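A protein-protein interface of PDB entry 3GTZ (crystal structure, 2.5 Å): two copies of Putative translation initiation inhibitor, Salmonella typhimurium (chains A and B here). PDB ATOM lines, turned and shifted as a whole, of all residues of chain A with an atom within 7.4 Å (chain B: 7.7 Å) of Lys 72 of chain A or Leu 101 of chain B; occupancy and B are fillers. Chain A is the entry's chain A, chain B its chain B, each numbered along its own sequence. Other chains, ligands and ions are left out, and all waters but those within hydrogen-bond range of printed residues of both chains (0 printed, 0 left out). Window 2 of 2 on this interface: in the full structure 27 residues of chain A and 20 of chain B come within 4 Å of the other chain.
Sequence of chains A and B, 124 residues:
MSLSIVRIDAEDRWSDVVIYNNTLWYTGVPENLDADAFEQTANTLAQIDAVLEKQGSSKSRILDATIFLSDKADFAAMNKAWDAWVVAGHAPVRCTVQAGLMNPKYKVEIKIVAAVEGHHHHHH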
ATOM      1  N   LEU A  69      13.978  28.192 -23.907  1.00  0.00           N
ATOM      2  CA  LEU A  69      13.350  27.675 -25.133  1.00  0.00           C
ATOM      3  C   LEU A  69      13.401  26.177 -25.077  1.00  0.00           C
ATOM      4  O   LEU A  69      14.401  25.628 -24.653  1.00  0.00           O
ATOM      5  CB  LEU A  69      14.133  28.141 -26.357  1.00  0.00           C
ATOM      6  CG  LEU A  69      14.117  29.637 -26.659  1.00  0.00           C
ATOM      7  CD1 LEU A  69      15.305  29.985 -27.504  1.00  0.00           C
ATOM      8  CD2 LEU A  69      12.809  30.096 -27.329  1.00  0.00           C
ATOM      9  N   SER A  70      12.355  25.514 -25.532  1.00  0.00           N
ATOM     10  CA  SER A  70      12.365  24.063 -25.618  1.00  0.00           C
ATOM     11  C   SER A  70      13.237  23.503 -26.768  1.00  0.00           C
ATOM     12  O   SER A  70      13.665  22.345 -26.723  1.00  0.00           O
ATOM     13  CB  SER A  70      10.931  23.537 -25.725  1.00  0.00           C
ATOM     14  OG  SER A  70      10.350  23.892 -26.947  1.00  0.00           O
ATOM     15  N   ASP A  71      13.523  24.333 -27.771  1.00  0.00           N
ATOM     16  CA  ASP A  71      14.179  23.878 -28.987  1.00  0.00           C
ATOM     17  C   ASP A  71      15.133  24.961 -29.435  1.00  0.00           C
ATOM     18  O   ASP A  71      14.790  26.126 -29.444  1.00  0.00           O
ATOM     19  CB  ASP A  71      13.140  23.589 -30.076  1.00  0.00           C
ATOM     20  CG  ASP A  71      13.603  22.556 -31.099  1.00  0.00           C
ATOM     21  OD1 ASP A  71      14.835  22.450 -31.366  1.00  0.00           O
ATOM     22  OD2 ASP A  71      12.721  21.870 -31.680  1.00  0.00           O
ATOM     23  N   LYS A  72      16.334  24.548 -29.807  1.00  0.00           N
ATOM     24  CA  LYS A  72      17.412  25.416 -30.201  1.00  0.00           C
ATOM     25  C   LYS A  72      17.080  26.059 -31.556  1.00  0.00           C
ATOM     26  O   LYS A  72      17.609  27.129 -31.878  1.00  0.00           O
ATOM     27  CB  LYS A  72      18.710  24.579 -30.318  1.00  0.00           C
ATOM     28  CG  LYS A  72      19.956  25.167 -29.651  1.00  0.00           C
ATOM     29  CD  LYS A  72      20.875  24.076 -29.028  1.00  0.00           C
ATOM     30  CE  LYS A  72      22.370  24.435 -29.135  1.00  0.00           C
ATOM     31  NZ  LYS A  72      23.236  23.373 -28.549  1.00  0.00           N
ATOM     32  N   ALA A  73      16.230  25.389 -32.338  1.00  0.00           N
ATOM     33  CA  ALA A  73      15.760  25.899 -33.631  1.00  0.00           C
ATOM     34  C   ALA A  73      14.847  27.163 -33.519  1.00  0.00           C
ATOM     35  O   ALA A  73      14.569  27.840 -34.523  1.00  0.00           O
ATOM     36  CB  ALA A  73      15.002  24.767 -34.401  1.00  0.00           C
ATOM     37  N   ASP A  74      14.384  27.464 -32.306  1.00  0.00           N
ATOM     38  CA  ASP A  74      13.495  28.598 -32.066  1.00  0.00           C
ATOM     39  C   ASP A  74      14.223  29.862 -31.648  1.00  0.00           C
ATOM     40  O   ASP A  74      13.589  30.884 -31.528  1.00  0.00           O
ATOM     41  CB  ASP A  74      12.416  28.219 -31.041  1.00  0.00           C
ATOM     42  CG  ASP A  74      11.345  27.332 -31.642  1.00  0.00           C
ATOM     43  OD1 ASP A  74      11.139  27.413 -32.880  1.00  0.00           O
ATOM     44  OD2 ASP A  74      10.709  26.556 -30.893  1.00  0.00           O
ATOM     45  N   PHE A  75      15.541  29.808 -31.479  1.00  0.00           N
ATOM     46  CA  PHE A  75      16.338  31.011 -31.131  1.00  0.00           C
ATOM     47  C   PHE A  75      16.040  32.259 -32.012  1.00  0.00           C
ATOM     48  O   PHE A  75      15.918  33.376 -31.497  1.00  0.00           O
ATOM     49  CB  PHE A  75      17.848  30.728 -31.204  1.00  0.00           C
ATOM     50  CG  PHE A  75      18.431  30.007 -29.992  1.00  0.00           C
ATOM     51  CD1 PHE A  75      18.148  30.403 -28.698  1.00  0.00           C
ATOM     52  CD2 PHE A  75      19.349  28.966 -30.156  1.00  0.00           C
ATOM     53  CE1 PHE A  75      18.735  29.748 -27.580  1.00  0.00           C
ATOM     54  CE2 PHE A  75      19.932  28.317 -29.043  1.00  0.00           C
ATOM     55  CZ  PHE A  75      19.611  28.709 -27.764  1.00  0.00           C
ATOM     56  N   ALA A  76      15.942  32.081 -33.325  1.00  0.00           N
ATOM     57  CA  ALA A  76      15.801  33.216 -34.234  1.00  0.00           C
ATOM     58  C   ALA A  76      14.410  33.793 -34.111  1.00  0.00           C
ATOM     59  O   ALA A  76      14.239  34.999 -34.144  1.00  0.00           O
ATOM     60  CB  ALA A  76      16.107  32.827 -35.733  1.00  0.00           C
ATOM     61  N   THR A  96      19.629  33.574 -22.620  1.00  0.00           N
ATOM     62  CA  THR A  96      18.799  32.599 -23.293  1.00  0.00           C
ATOM     63  C   THR A  96      19.444  31.224 -23.272  1.00  0.00           C
ATOM     64  O   THR A  96      20.596  31.081 -23.666  1.00  0.00           O
ATOM     65  CB  THR A  96      18.588  32.993 -24.750  1.00  0.00           C
ATOM     66  OG1 THR A  96      18.243  34.379 -24.814  1.00  0.00           O
ATOM     67  CG2 THR A  96      17.473  32.207 -25.351  1.00  0.00           C
ATOM     68  N   VAL A  97      18.694  30.221 -22.819  1.00  0.00           N
ATOM     69  CA  VAL A  97      19.142  28.837 -22.821  1.00  0.00           C
ATOM     70  C   VAL A  97      18.025  27.903 -23.228  1.00  0.00           C
ATOM     71  O   VAL A  97      16.861  28.235 -23.075  1.00  0.00           O
ATOM     72  CB  VAL A  97      19.600  28.402 -21.438  1.00  0.00           C
ATOM     73  CG1 VAL A  97      20.685  29.332 -20.933  1.00  0.00           C
ATOM     74  CG2 VAL A  97      18.397  28.324 -20.462  1.00  0.00           C
ATOM     75  N   GLN A  98      18.387  26.712 -23.707  1.00  0.00           N
ATOM     76  CA  GLN A  98      17.407  25.711 -24.144  1.00  0.00           C
ATOM     77  C   GLN A  98      17.267  24.665 -23.080  1.00  0.00           C
ATOM     78  O   GLN A  98      18.232  24.171 -22.597  1.00  0.00           O
ATOM     79  CB  GLN A  98      17.849  25.056 -25.437  1.00  0.00           C
ATOM     80  CG  GLN A  98      16.864  24.051 -25.985  1.00  0.00           C
ATOM     81  CD  GLN A  98      17.086  22.666 -25.445  1.00  0.00           C
ATOM     82  OE1 GLN A  98      18.205  22.278 -25.174  1.00  0.00           O
ATOM     83  NE2 GLN A  98      16.018  21.911 -25.294  1.00  0.00           N
ATOM     84  N   ALA A  99      16.049  24.335 -22.711  1.00  0.00           N
ATOM     85  CA  ALA A  99      15.801  23.409 -21.625  1.00  0.00           C
ATOM     86  C   ALA A  99      14.438  22.758 -21.808  1.00  0.00           C
ATOM     87  O   ALA A  99      13.650  23.171 -22.660  1.00  0.00           O
ATOM     88  CB  ALA A  99      15.880  24.129 -20.307  1.00  0.00           C
ATOM     89  N   PRO B  30      32.183  33.286 -22.280  1.00  0.00           N
ATOM     90  CA  PRO B  30      33.626  33.210 -22.530  1.00  0.00           C
ATOM     91  C   PRO B  30      33.996  33.924 -23.845  1.00  0.00           C
ATOM     92  O   PRO B  30      33.197  33.936 -24.796  1.00  0.00           O
ATOM     93  CB  PRO B  30      33.878  31.708 -22.632  1.00  0.00           C
ATOM     94  CG  PRO B  30      32.579  31.125 -23.135  1.00  0.00           C
ATOM     95  CD  PRO B  30      31.493  32.009 -22.565  1.00  0.00           C
ATOM     96  N   GLN B  40      37.460  28.049 -20.594  1.00  0.00           N
ATOM     97  CA  GLN B  40      36.321  28.961 -20.868  1.00  0.00           C
ATOM     98  C   GLN B  40      35.667  29.452 -19.577  1.00  0.00           C
ATOM     99  O   GLN B  40      35.270  30.612 -19.471  1.00  0.00           O
ATOM    100  CB  GLN B  40      35.277  28.310 -21.772  1.00  0.00           C
ATOM    101  CG  GLN B  40      35.582  28.476 -23.260  1.00  0.00           C
ATOM    102  CD  GLN B  40      34.502  27.934 -24.194  1.00  0.00           C
ATOM    103  OE1 GLN B  40      33.314  27.941 -23.869  1.00  0.00           O
ATOM    104  NE2 GLN B  40      34.914  27.483 -25.372  1.00  0.00           N
ATOM    105  N   ILE B  67      25.521  28.557 -13.106  1.00  0.00           N
ATOM    106  CA  ILE B  67      26.469  28.189 -14.120  1.00  0.00           C
ATOM    107  C   ILE B  67      25.735  27.251 -15.042  1.00  0.00           C
ATOM    108  O   ILE B  67      25.261  26.228 -14.580  1.00  0.00           O
ATOM    109  CB  ILE B  67      27.664  27.491 -13.481  1.00  0.00           C
ATOM    110  CG1 ILE B  67      28.253  28.395 -12.378  1.00  0.00           C
ATOM    111  CG2 ILE B  67      28.723  27.096 -14.528  1.00  0.00           C
ATOM    112  CD1 ILE B  67      29.616  27.933 -11.839  1.00  0.00           C
ATOM    113  N   PHE B  68      25.597  27.616 -16.324  1.00  0.00           N
ATOM    114  CA  PHE B  68      25.037  26.719 -17.347  1.00  0.00           C
ATOM    115  C   PHE B  68      26.160  26.068 -18.145  1.00  0.00           C
ATOM    116  O   PHE B  68      27.053  26.738 -18.641  1.00  0.00           O
ATOM    117  CB  PHE B  68      24.123  27.476 -18.298  1.00  0.00           C
ATOM    118  CG  PHE B  68      22.939  28.049 -17.636  1.00  0.00           C
ATOM    119  CD1 PHE B  68      21.835  27.256 -17.365  1.00  0.00           C
ATOM    120  CD2 PHE B  68      22.914  29.380 -17.256  1.00  0.00           C
ATOM    121  CE1 PHE B  68      20.717  27.773 -16.750  1.00  0.00           C
ATOM    122  CE2 PHE B  68      21.785  29.915 -16.625  1.00  0.00           C
ATOM    123  CZ  PHE B  68      20.690  29.104 -16.373  1.00  0.00           C
ATOM    124  N   LEU B  69      26.129  24.750 -18.246  1.00  0.00           N
ATOM    125  CA  LEU B  69      27.123  24.019 -19.030  1.00  0.00           C
ATOM    126  C   LEU B  69      26.412  23.429 -20.225  1.00  0.00           C
ATOM    127  O   LEU B  69      25.270  23.000 -20.108  1.00  0.00           O
ATOM    128  CB  LEU B  69      27.769  22.907 -18.207  1.00  0.00           C
ATOM    129  CG  LEU B  69      28.743  23.334 -17.111  1.00  0.00           C
ATOM    130  CD1 LEU B  69      29.354  22.118 -16.421  1.00  0.00           C
ATOM    131  CD2 LEU B  69      29.843  24.216 -17.663  1.00  0.00           C
ATOM    132  N   SER B  70      27.083  23.422 -21.371  1.00  0.00           N
ATOM    133  CA  SER B  70      26.519  22.815 -22.569  1.00  0.00           C
ATOM    134  C   SER B  70      26.543  21.302 -22.535  1.00  0.00           C
ATOM    135  O   SER B  70      25.702  20.673 -23.147  1.00  0.00           O
ATOM    136  CB  SER B  70      27.257  23.294 -23.831  1.00  0.00           C
ATOM    137  OG  SER B  70      28.543  22.705 -23.906  1.00  0.00           O
ATOM    138  N   ASP B  71      27.522  20.732 -21.838  1.00  0.00           N
ATOM    139  CA  ASP B  71      27.816  19.282 -21.893  1.00  0.00           C
ATOM    140  C   ASP B  71      27.982  18.731 -20.487  1.00  0.00           C
ATOM    141  O   ASP B  71      28.736  19.278 -19.690  1.00  0.00           O
ATOM    142  CB  ASP B  71      29.107  19.034 -22.699  1.00  0.00           C
ATOM    143  CG  ASP B  71      29.245  17.586 -23.196  1.00  0.00           C
ATOM    144  OD1 ASP B  71      29.029  16.614 -22.404  1.00  0.00           O
ATOM    145  OD2 ASP B  71      29.594  17.421 -24.403  1.00  0.00           O
ATOM    146  N   VAL B  97      24.079  23.652 -13.741  1.00  0.00           N
ATOM    147  CA  VAL B  97      23.278  22.710 -14.517  1.00  0.00           C
ATOM    148  C   VAL B  97      23.663  22.663 -15.991  1.00  0.00           C
ATOM    149  O   VAL B  97      24.357  23.532 -16.493  1.00  0.00           O
ATOM    150  CB  VAL B  97      21.765  23.030 -14.462  1.00  0.00           C
ATOM    151  CG1 VAL B  97      21.282  23.151 -13.022  1.00  0.00           C
ATOM    152  CG2 VAL B  97      21.437  24.271 -15.267  1.00  0.00           C
ATOM    153  N   GLN B  98      23.185  21.636 -16.679  1.00  0.00           N
ATOM    154  CA  GLN B  98      23.440  21.455 -18.087  1.00  0.00           C
ATOM    155  C   GLN B  98      22.226  21.857 -18.899  1.00  0.00           C
ATOM    156  O   GLN B  98      21.142  21.330 -18.688  1.00  0.00           O
ATOM    157  CB  GLN B  98      23.783  19.998 -18.395  1.00  0.00           C
ATOM    158  CG  GLN B  98      24.109  19.726 -19.860  1.00  0.00           C
ATOM    159  CD  GLN B  98      22.895  19.225 -20.653  1.00  0.00           C
ATOM    160  OE1 GLN B  98      22.094  18.428 -20.146  1.00  0.00           O
ATOM    161  NE2 GLN B  98      22.747  19.707 -21.896  1.00  0.00           N
ATOM    162  N   ALA B  99      22.419  22.771 -19.837  1.00  0.00           N
ATOM    163  CA  ALA B  99      21.395  23.099 -20.803  1.00  0.00           C
ATOM    164  C   ALA B  99      22.048  23.526 -22.121  1.00  0.00           C
ATOM    165  O   ALA B  99      23.265  23.759 -22.179  1.00  0.00           O
ATOM    166  CB  ALA B  99      20.527  24.206 -20.251  1.00  0.00           C
ATOM    167  N   GLY B 100      21.248  23.614 -23.178  1.00  0.00           N
ATOM    168  CA  GLY B 100      21.722  24.130 -24.453  1.00  0.00           C
ATOM    169  C   GLY B 100      22.044  25.624 -24.404  1.00  0.00           C
ATOM    170  O   GLY B 100      21.251  26.441 -23.897  1.00  0.00           O
ATOM    171  N   LEU B 101      23.207  25.989 -24.936  1.00  0.00           N
ATOM    172  CA  LEU B 101      23.633  27.389 -25.000  1.00  0.00           C
ATOM    173  C   LEU B 101      23.422  27.930 -26.423  1.00  0.00           C
ATOM    174  O   LEU B 101      23.199  27.149 -27.335  1.00  0.00           O
ATOM    175  CB  LEU B 101      25.080  27.509 -24.524  1.00  0.00           C
ATOM    176  CG  LEU B 101      25.319  27.590 -23.002  1.00  0.00           C
ATOM    177  CD1 LEU B 101      24.233  26.943 -22.152  1.00  0.00           C
ATOM    178  CD2 LEU B 101      26.665  27.000 -22.646  1.00  0.00           C
ATOM    179  N   MET B 102      23.456  29.246 -26.608  1.00  0.00           N
ATOM    180  CA  MET B 102      23.046  29.852 -27.887  1.00  0.00           C
ATOM    181  C   MET B 102      24.131  29.756 -28.968  1.00  0.00           C
ATOM    182  O   MET B 102      23.856  29.404 -30.114  1.00  0.00           O
ATOM    183  CB  MET B 102      22.583  31.318 -27.700  1.00  0.00           C
ATOM    184  CG  MET B 102      22.097  32.004 -29.018  1.00  0.00           C
ATOM    185  SD  MET B 102      21.028  33.508 -28.893  1.00  0.00           S
ATOM    186  CE  MET B 102      21.110  34.012 -30.628  1.00  0.00           C
ATOM    187  N   ASN B 103      25.361  30.075 -28.597  1.00  0.00           N
ATOM    188  CA  ASN B 103      26.492  29.896 -29.487  1.00  0.00           C
ATOM    189  C   ASN B 103      27.032  28.476 -29.338  1.00  0.00           C
ATOM    190  O   ASN B 103      27.377  28.078 -28.232  1.00  0.00           O
ATOM    191  CB  ASN B 103      27.580  30.912 -29.138  1.00  0.00           C
ATOM    192  CG  ASN B 103      28.557  31.125 -30.275  1.00  0.00           C
ATOM    193  OD1 ASN B 103      29.209  30.173 -30.727  1.00  0.00           O
ATOM    194  ND2 ASN B 103      28.658  32.375 -30.755  1.00  0.00           N
ATOM    195  N   PRO B 104      27.113  27.706 -30.435  1.00  0.00           N
ATOM    196  CA  PRO B 104      27.558  26.297 -30.318  1.00  0.00           C
ATOM    197  C   PRO B 104      28.981  26.081 -29.815  1.00  0.00           C
ATOM    198  O   PRO B 104      29.339  24.963 -29.444  1.00  0.00           O
ATOM    199  CB  PRO B 104      27.387  25.727 -31.736  1.00  0.00           C
ATOM    200  CG  PRO B 104      27.213  26.944 -32.644  1.00  0.00           C
ATOM    201  CD  PRO B 104      26.743  28.085 -31.814  1.00  0.00           C
ATOM    202  N   LYS B 105      29.783  27.137 -29.789  1.00  0.00           N
ATOM    203  CA  LYS B 105      31.124  27.046 -29.213  1.00  0.00           C
ATOM    204  C   LYS B 105      31.164  27.405 -27.705  1.00  0.00           C
ATOM    205  O   LYS B 105      32.242  27.412 -27.101  1.00  0.00           O
ATOM    206  CB  LYS B 105      32.107  27.918 -30.015  1.00  0.00           C
ATOM    207  CG  LYS B 105      32.274  27.484 -31.515  1.00  0.00           C
ATOM    208  CD  LYS B 105      33.776  27.448 -31.969  1.00  0.00           C
ATOM    209  CE  LYS B 105      34.031  28.147 -33.340  1.00  0.00           C
ATOM    210  NZ  LYS B 105      34.019  29.673 -33.256  1.00  0.00           N
ATOM    211  N   TYR B 106      29.999  27.701 -27.108  1.00  0.00           N
ATOM    212  CA  TYR B 106      29.906  27.922 -25.658  1.00  0.00           C
ATOM    213  C   TYR B 106      29.943  26.604 -24.897  1.00  0.00           C
ATOM    214  O   TYR B 106      29.102  25.726 -25.137  1.00  0.00           O
ATOM    215  CB  TYR B 106      28.619  28.668 -25.288  1.00  0.00           C
ATOM    216  CG  TYR B 106      28.561  30.101 -25.727  1.00  0.00           C
ATOM    217  CD1 TYR B 106      29.687  30.764 -26.197  1.00  0.00           C
ATOM    218  CD2 TYR B 106      27.385  30.814 -25.640  1.00  0.00           C
ATOM    219  CE1 TYR B 106      29.628  32.099 -26.596  1.00  0.00           C
ATOM    220  CE2 TYR B 106      27.318  32.153 -26.034  1.00  0.00           C
ATOM    221  CZ  TYR B 106      28.447  32.785 -26.516  1.00  0.00           C
ATOM    222  OH  TYR B 106      28.412  34.093 -26.918  1.00  0.00           O
ATOM    223  N   LYS B 107      30.926  26.455 -24.010  1.00  0.00           N
ATOM    224  CA  LYS B 107      30.922  25.319 -23.096  1.00  0.00           C
ATOM    225  C   LYS B 107      30.182  25.750 -21.854  1.00  0.00           C
ATOM    226  O   LYS B 107      29.514  24.937 -21.234  1.00  0.00           O
ATOM    227  CB  LYS B 107      32.334  24.838 -22.718  1.00  0.00           C
ATOM    228  CG  LYS B 107      33.202  24.207 -23.860  1.00  0.00           C
ATOM    229  CD  LYS B 107      32.433  23.227 -24.755  1.00  0.00           C
ATOM    230  CE  LYS B 107      33.382  22.286 -25.595  1.00  0.00           C
ATOM    231  NZ  LYS B 107      34.588  22.948 -26.192  1.00  0.00           N
ATOM    232  N   VAL B 108      30.276  27.048 -21.533  1.00  0.00           N
ATOM    233  CA  VAL B 108      29.816  27.596 -20.278  1.00  0.00           C
ATOM    234  C   VAL B 108      29.236  29.015 -20.406  1.00  0.00           C
ATOM    235  O   VAL B 108      29.587  29.757 -21.314  1.00  0.00           O
ATOM    236  CB  VAL B 108      30.977  27.614 -19.267  1.00  0.00           C
ATOM    237  CG1 VAL B 108      31.996  28.669 -19.651  1.00  0.00           C
ATOM    238  CG2 VAL B 108      30.455  27.860 -17.864  1.00  0.00           C
ATOM    239  N   GLU B 109      28.371  29.376 -19.454  1.00  0.00           N
ATOM    240  CA  GLU B 109      27.743  30.697 -19.352  1.00  0.00           C
ATOM    241  C   GLU B 109      27.316  30.924 -17.886  1.00  0.00           C
ATOM    242  O   GLU B 109      26.666  30.062 -17.290  1.00  0.00           O
ATOM    243  CB  GLU B 109      26.517  30.710 -20.268  1.00  0.00           C
ATOM    244  CG  GLU B 109      26.014  32.058 -20.679  1.00  0.00           C
ATOM    245  CD  GLU B 109      25.056  32.003 -21.880  1.00  0.00           C
ATOM    246  OE1 GLU B 109      24.128  32.843 -21.895  1.00  0.00           O
ATOM    247  OE2 GLU B 109      25.216  31.140 -22.797  1.00  0.00           O
ATOM    248  N   ILE B 110      27.688  32.054 -17.304  1.00  0.00           N
ATOM    249  CA  ILE B 110      27.549  32.256 -15.860  1.00  0.00           C
ATOM    250  C   ILE B 110      26.773  33.524 -15.542  1.00  0.00           C
ATOM    251  O   ILE B 110      27.203  34.625 -15.869  1.00  0.00           O
ATOM    252  CB  ILE B 110      28.916  32.354 -15.142  1.00  0.00           C
ATOM    253  CG1 ILE B 110      29.779  31.113 -15.408  1.00  0.00           C
ATOM    254  CG2 ILE B 110      28.731  32.523 -13.677  1.00  0.00           C
ATOM    255  CD1 ILE B 110      31.204  31.297 -15.039  1.00  0.00           C
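O of Leu 101 of chain B touches CE of Lys 72 of chain A, 3.4 Å away. Phe 75 of chain A touches Leu 101 of chain B. Phe 75 of chain A touches Met 102 of chain B (CZ to CA, 3.6 Å). Gly 100 of chain B touches Val 97 of chain A. Gln 98 of chain A touches Ala 99 of chain B (O to CB, 3.3 Å).
Of the 21 printed residues of chain B, 4 touch a printed residue of chain A. Hydrophobic or aromatic side chains of chain B that line the printed part of chain A: Ala 99 and Met 102. Of the 12 printed residues of chain A, 4 touch a printed residue of chain B. Printed residues of chain A that touch a printed residue of chain B: Lys 72, Phe 75, Val 97 and Gln 98. Hydrophobic or aromatic side chains of chain A within 4 Å of the printed part of chain B: Phe 75 and Val 97. Among the printed residues, 6 pairs touch across the chains. Among the printed residues, no Asp or Glu carboxylate lies within 4 Å of a Lys or Arg side-chain nitrogen of the other chain.
The backbone NH (N) of Leu 69 of chain A sits at hydrogen-bond distance from the backbone carbonyl oxygen (O) of Val 97 of chain A (3.0 Å). O of Leu 69 of chain B lies within hydrogen-bond range of N of Ala 99 of chain B (2.9 Å). The side-chain amide nitrogen (NE2) of Gln 98 of chain A is in hydrogen-bond range of the backbone carbonyl oxygen (O) of Ser 70 of chain A, at 2.8 Å.
Lys 72 of chain A touches one residue of chain B. Of the printed residues of chain B, Phe 75 of chain A touches Leu 101 and Met 102. Of the printed residues of chain B, Val 97 of chain A touches Gly 100 (3.4 Å). Of the printed residues of chain A, Ala 99 of chain B touches Gln 98 (3.3 Å).
N of Gln 98 of chain A is in hydrogen-bond range of O of Gly 100 of chain B.
Gln 98 of chain A touches Ala 99 of chain B, but with the chains exchanged Ala 99 of chain A does not touch Gln 98 of chain B (6.2 Å).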
